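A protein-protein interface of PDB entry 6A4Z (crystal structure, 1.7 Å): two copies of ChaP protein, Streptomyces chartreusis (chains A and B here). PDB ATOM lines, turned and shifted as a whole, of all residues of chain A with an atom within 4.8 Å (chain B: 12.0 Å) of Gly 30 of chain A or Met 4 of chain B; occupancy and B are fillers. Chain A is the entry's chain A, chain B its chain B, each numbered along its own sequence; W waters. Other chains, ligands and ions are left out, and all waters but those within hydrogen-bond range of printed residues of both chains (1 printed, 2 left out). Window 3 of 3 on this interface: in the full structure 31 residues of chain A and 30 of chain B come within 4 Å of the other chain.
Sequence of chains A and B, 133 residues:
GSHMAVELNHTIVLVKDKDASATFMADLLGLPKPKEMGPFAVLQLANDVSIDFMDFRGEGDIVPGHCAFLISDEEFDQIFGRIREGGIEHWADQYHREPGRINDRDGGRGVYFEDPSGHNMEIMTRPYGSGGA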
ATOM      1  N   MET A  25     -29.407  32.012  31.595  1.00  0.00           N
ATOM      2  CA  MET A  25     -29.398  30.619  31.161  1.00  0.00           C
ATOM      3  C   MET A  25     -28.459  30.392  29.972  1.00  0.00           C
ATOM      4  O   MET A  25     -27.746  29.387  29.932  1.00  0.00           O
ATOM      5  CB  MET A  25     -30.829  30.170  30.815  1.00  0.00           C
ATOM      6  CG  MET A  25     -31.766  30.127  32.035  1.00  0.00           C
ATOM      7  SD  MET A  25     -31.147  28.960  33.487  1.00  0.00           S
ATOM      8  CE  MET A  25     -31.412  27.236  32.620  1.00  0.00           C
ATOM      9  N   ALA A  26     -28.457  31.318  29.007  1.00  0.00           N
ATOM     10  CA  ALA A  26     -27.568  31.164  27.857  1.00  0.00           C
ATOM     11  C   ALA A  26     -26.112  31.259  28.280  1.00  0.00           C
ATOM     12  O   ALA A  26     -25.275  30.456  27.844  1.00  0.00           O
ATOM     13  CB  ALA A  26     -27.877  32.215  26.793  1.00  0.00           C
ATOM     14  N   ASP A  27     -25.785  32.254  29.113  1.00  0.00           N
ATOM     15  CA  ASP A  27     -24.418  32.388  29.616  1.00  0.00           C
ATOM     16  C   ASP A  27     -23.994  31.141  30.375  1.00  0.00           C
ATOM     17  O   ASP A  27     -22.894  30.613  30.167  1.00  0.00           O
ATOM     18  CB  ASP A  27     -24.308  33.623  30.505  1.00  0.00           C
ATOM     19  CG  ASP A  27     -24.271  34.912  29.712  1.00  0.00           C
ATOM     20  OD1 ASP A  27     -24.222  34.863  28.461  1.00  0.00           O
ATOM     21  OD2 ASP A  27     -24.308  35.983  30.346  1.00  0.00           O
ATOM     22  N   LEU A  28     -24.858  30.659  31.270  1.00  0.00           N
ATOM     23  CA  LEU A  28     -24.504  29.520  32.102  1.00  0.00           C
ATOM     24  C   LEU A  28     -24.381  28.243  31.279  1.00  0.00           C
ATOM     25  O   LEU A  28     -23.396  27.509  31.403  1.00  0.00           O
ATOM     26  CB  LEU A  28     -25.541  29.356  33.209  1.00  0.00           C
ATOM     27  CG  LEU A  28     -25.210  28.233  34.176  1.00  0.00           C
ATOM     28  CD1 LEU A  28     -23.820  28.470  34.798  1.00  0.00           C
ATOM     29  CD2 LEU A  28     -26.287  28.085  35.244  1.00  0.00           C
ATOM     30  N   LEU A  29     -25.351  27.979  30.400  1.00  0.00           N
ATOM     31  CA  LEU A  29     -25.344  26.745  29.624  1.00  0.00           C
ATOM     32  C   LEU A  29     -24.421  26.800  28.411  1.00  0.00           C
ATOM     33  O   LEU A  29     -24.264  25.778  27.732  1.00  0.00           O
ATOM     34  CB  LEU A  29     -26.776  26.400  29.177  1.00  0.00           C
ATOM     35  CG  LEU A  29     -27.772  26.096  30.310  1.00  0.00           C
ATOM     36  CD1 LEU A  29     -29.193  25.944  29.757  1.00  0.00           C
ATOM     37  CD2 LEU A  29     -27.374  24.855  31.122  1.00  0.00           C
ATOM     38  N   GLY A  30     -23.823  27.956  28.118  1.00  0.00           N
ATOM     39  CA  GLY A  30     -22.959  28.124  26.964  1.00  0.00           C
ATOM     40  C   GLY A  30     -23.696  28.036  25.642  1.00  0.00           C
ATOM     41  O   GLY A  30     -23.256  27.343  24.718  1.00  0.00           O
ATOM     42  N   LEU A  31     -24.810  28.751  25.535  1.00  0.00           N
ATOM     43  CA  LEU A  31     -25.653  28.776  24.351  1.00  0.00           C
ATOM     44  C   LEU A  31     -25.602  30.142  23.679  1.00  0.00           C
ATOM     45  O   LEU A  31     -25.151  31.126  24.276  1.00  0.00           O
ATOM     46  CB  LEU A  31     -27.103  28.447  24.734  1.00  0.00           C
ATOM     47  CG  LEU A  31     -27.267  27.069  25.381  1.00  0.00           C
ATOM     48  CD1 LEU A  31     -28.687  26.883  25.894  1.00  0.00           C
ATOM     49  CD2 LEU A  31     -26.877  25.958  24.419  1.00  0.00           C
ATOM     50  N   PRO A  32     -26.059  30.240  22.432  1.00  0.00           N
ATOM     51  CA  PRO A  32     -26.119  31.546  21.769  1.00  0.00           C
ATOM     52  C   PRO A  32     -27.012  32.522  22.519  1.00  0.00           C
ATOM     53  O   PRO A  32     -27.898  32.138  23.289  1.00  0.00           O
ATOM     54  CB  PRO A  32     -26.685  31.220  20.382  1.00  0.00           C
ATOM     55  CG  PRO A  32     -27.151  29.812  20.448  1.00  0.00           C
ATOM     56  CD  PRO A  32     -26.335  29.140  21.498  1.00  0.00           C
ATOM     57  N   GLU A  75     -19.444  19.074  28.851  1.00  0.00           N
ATOM     58  CA  GLU A  75     -20.292  20.227  29.119  1.00  0.00           C
ATOM     59  C   GLU A  75     -20.606  20.352  30.602  1.00  0.00           C
ATOM     60  O   GLU A  75     -20.644  21.468  31.138  1.00  0.00           O
ATOM     61  CB  GLU A  75     -21.572  20.137  28.277  1.00  0.00           C
ATOM     62  CG  GLU A  75     -21.267  20.428  26.802  1.00  0.00           C
ATOM     63  CD  GLU A  75     -22.310  19.880  25.846  1.00  0.00           C
ATOM     64  OE1 GLU A  75     -23.156  19.070  26.284  1.00  0.00           O
ATOM     65  OE2 GLU A  75     -22.262  20.244  24.649  1.00  0.00           O
ATOM     66  N   GLN A  78     -17.713  22.096  32.324  1.00  0.00           N
ATOM     67  CA  GLN A  78     -17.634  23.528  32.054  1.00  0.00           C
ATOM     68  C   GLN A  78     -18.775  24.290  32.713  1.00  0.00           C
ATOM     69  O   GLN A  78     -18.553  25.345  33.319  1.00  0.00           O
ATOM     70  CB  GLN A  78     -17.604  23.774  30.549  1.00  0.00           C
ATOM     71  CG  GLN A  78     -16.392  23.152  29.880  1.00  0.00           C
ATOM     72  CD  GLN A  78     -16.355  23.399  28.388  1.00  0.00           C
ATOM     73  OE1 GLN A  78     -16.835  24.420  27.907  1.00  0.00           O
ATOM     74  NE2 GLN A  78     -15.827  22.441  27.642  1.00  0.00           N
ATOM     75  N   ILE A  79     -19.997  23.762  32.629  1.00  0.00           N
ATOM     76  CA  ILE A  79     -21.153  24.455  33.197  1.00  0.00           C
ATOM     77  C   ILE A  79     -21.082  24.474  34.722  1.00  0.00           C
ATOM     78  O   ILE A  79     -21.304  25.514  35.355  1.00  0.00           O
ATOM     79  CB  ILE A  79     -22.456  23.814  32.688  1.00  0.00           C
ATOM     80  CG1 ILE A  79     -22.584  24.026  31.180  1.00  0.00           C
ATOM     81  CG2 ILE A  79     -23.679  24.372  33.427  1.00  0.00           C
ATOM     82  CD1 ILE A  79     -23.720  23.229  30.531  1.00  0.00           C
ATOM     83  N   ARG A  82     -18.813  27.083  35.784  1.00  0.00           N
ATOM     84  CA  ARG A  82     -19.432  28.401  35.832  1.00  0.00           C
ATOM     85  C   ARG A  82     -20.329  28.568  37.053  1.00  0.00           C
ATOM     86  O   ARG A  82     -20.445  29.680  37.579  1.00  0.00           O
ATOM     87  CB  ARG A  82     -20.235  28.658  34.550  1.00  0.00           C
ATOM     88  CG  ARG A  82     -19.376  28.813  33.308  1.00  0.00           C
ATOM     89  CD  ARG A  82     -20.245  28.987  32.043  1.00  0.00           C
ATOM     90  NE  ARG A  82     -19.445  28.694  30.861  1.00  0.00           N
ATOM     91  CZ  ARG A  82     -19.724  27.755  29.966  1.00  0.00           C
ATOM     92  NH1 ARG A  82     -20.829  27.020  30.066  1.00  0.00           N
ATOM     93  NH2 ARG A  82     -18.906  27.586  28.940  1.00  0.00           N
ATOM     94  N   MET B   4     -22.615  24.786  23.016  1.00  0.00           N
ATOM     95  CA  MET B   4     -22.718  23.482  23.674  1.00  0.00           C
ATOM     96  C   MET B   4     -23.929  22.733  23.135  1.00  0.00           C
ATOM     97  O   MET B   4     -24.910  23.366  22.754  1.00  0.00           O
ATOM     98  CB  MET B   4     -22.807  23.671  25.182  1.00  0.00           C
ATOM     99  CG  MET B   4     -21.544  24.249  25.748  1.00  0.00           C
ATOM    100  SD  MET B   4     -21.470  24.147  27.674  1.00  0.00           S
ATOM    101  CE  MET B   4     -19.693  24.802  27.902  1.00  0.00           C
ATOM    102  N   ALA B   5     -23.849  21.404  23.022  1.00  0.00           N
ATOM    103  CA  ALA B   5     -25.009  20.637  22.565  1.00  0.00           C
ATOM    104  C   ALA B   5     -25.839  20.282  23.797  1.00  0.00           C
ATOM    105  O   ALA B   5     -25.899  19.144  24.269  1.00  0.00           O
ATOM    106  CB  ALA B   5     -24.575  19.403  21.786  1.00  0.00           C
ATOM    107  N   VAL B   6     -26.486  21.308  24.309  1.00  0.00           N
ATOM    108  CA  VAL B   6     -27.349  21.196  25.478  1.00  0.00           C
ATOM    109  C   VAL B   6     -28.757  20.868  25.007  1.00  0.00           C
ATOM    110  O   VAL B   6     -29.310  21.576  24.163  1.00  0.00           O
ATOM    111  CB  VAL B   6     -27.336  22.500  26.292  1.00  0.00           C
ATOM    112  CG1 VAL B   6     -28.339  22.421  27.440  1.00  0.00           C
ATOM    113  CG2 VAL B   6     -25.919  22.794  26.806  1.00  0.00           C
ATOM    114  N   GLU B   7     -29.336  19.795  25.534  1.00  0.00           N
ATOM    115  CA  GLU B   7     -30.705  19.413  25.189  1.00  0.00           C
ATOM    116  C   GLU B   7     -31.654  19.715  26.334  1.00  0.00           C
ATOM    117  O   GLU B   7     -31.317  19.511  27.496  1.00  0.00           O
ATOM    118  CB  GLU B   7     -30.811  17.923  24.866  1.00  0.00           C
ATOM    119  CG  GLU B   7     -30.020  17.499  23.658  1.00  0.00           C
ATOM    120  CD  GLU B   7     -30.138  16.011  23.390  1.00  0.00           C
ATOM    121  OE1 GLU B   7     -29.710  15.568  22.313  1.00  0.00           O
ATOM    122  OE2 GLU B   7     -30.658  15.283  24.260  1.00  0.00           O
ATOM    123  N   LEU B   8     -32.867  20.151  25.997  1.00  0.00           N
ATOM    124  CA  LEU B   8     -33.946  20.181  26.976  1.00  0.00           C
ATOM    125  C   LEU B   8     -34.505  18.769  27.089  1.00  0.00           C
ATOM    126  O   LEU B   8     -35.021  18.223  26.109  1.00  0.00           O
ATOM    127  CB  LEU B   8     -35.039  21.159  26.547  1.00  0.00           C
ATOM    128  CG  LEU B   8     -36.259  21.131  27.481  1.00  0.00           C
ATOM    129  CD1 LEU B   8     -35.868  21.584  28.866  1.00  0.00           C
ATOM    130  CD2 LEU B   8     -37.400  22.009  26.927  1.00  0.00           C
HETATM  131  O   HOH W   1     -20.053  27.152  25.894  1.00  0.00           O
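Of the 5 printed residues of chain B, 3 touch a printed residue of chain A.
Hydrophobic or aromatic side chains of chain B within 4 Å of the printed part of chain A: Met 4, Ala 5 and Val 6.
Along chain B the printed residues that touch a printed residue of chain A span positions 4 to 6.
Among the printed residues, 10 pairs touch across the chains.
Among the printed residues, no Asp or Glu carboxylate lies within 4 Å of a Lys or Arg side-chain nitrogen of the other chain.
The backbone carbonyl oxygen (O) of Gly 30 of chain A lies within hydrogen-bond range of the backbone NH (N) of Met 4 of chain B (3.1 Å).
The side-chain carboxylate (OE2) of Glu 75 of chain A is in hydrogen-bond range of the backbone NH (N) of Ala 5 of chain B, 2.6 Å away.
The guanidinium group (NH1) of Arg 82 of chain A lies close to the side-chain sulfur (SD) of Met 4 of chain B (3.8 Å).
SD of Met 4 of chain B lies close to O of Leu 29 of chain A, 3.2 Å away.
No position is printed for both chains.
Of the 10 pairs that touch across the chains among the printed residues, none has its exchanged pair printed and touching as well.
Among the printed residues, pairs that only touch across the chains: Leu 29 of chain A with Val 6 of chain B, Leu 31 of chain A with Met 4 of chain B, Leu 31 of chain A with Val 6 of chain B, Glu 75 of chain A with Met 4 of chain B, Gln 78 of chain A with Met 4 of chain B and Ile 79 of chain A with Met 4 of chain B.
No residue of chain B comes within 4 Å of Leu 28 of chain A.
Of chain B, only Met 4 and Val 6 come within 4 Å of Leu 29 of chain A.
Gly 30 of chain A touches just one residue of chain B: Met 4.
Of the printed residues of chain B, Leu 31 of chain A touches Met 4 and Val 6.
No residue of chain B comes within 4 Å of Pro 32 of chain A.
Glu 75 of chain A touches just these residues of chain B: Met 4 (3.4 Å) and Ala 5 (2.6 Å).
Gln 78 of chain A touches just one residue of chain B: Met 4.
Of the printed residues of chain B, Ile 79 of chain A touches Met 4 (3.7 Å).
Of the printed residues of chain B, Arg 82 of chain A touches Met 4 (3.1 Å).
Met 4 of chain B touches just these residues of chain A: Leu 29 (3.2 Å), Gly 30 (3.1 Å), Leu 31 (3.7 Å), Glu 75 (3.4 Å), Gln 78 (2.9 Å), Ile 79 (3.7 Å) and Arg 82 (3.1 Å).
Printed residues of chain A within 4 Å of Ala 5 of chain B: Glu 75.
Printed residues of chain A within 4 Å of Val 6 of chain B: Leu 29 and Leu 31.
The backbone carbonyl oxygen (O) of Ala 26 of chain A is in hydrogen-bond range of the backbone NH (N) of Leu 31 of chain A (2.9 Å).
O of Leu 28 of chain A is in hydrogen-bond range of NH1 of Arg 82 of chain A (2.9 Å).
Water W1 lies within hydrogen-bond range of NH2 of Arg 82 of chain A, O of Gly 30 of chain A and SD of Met 4 of chain B.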
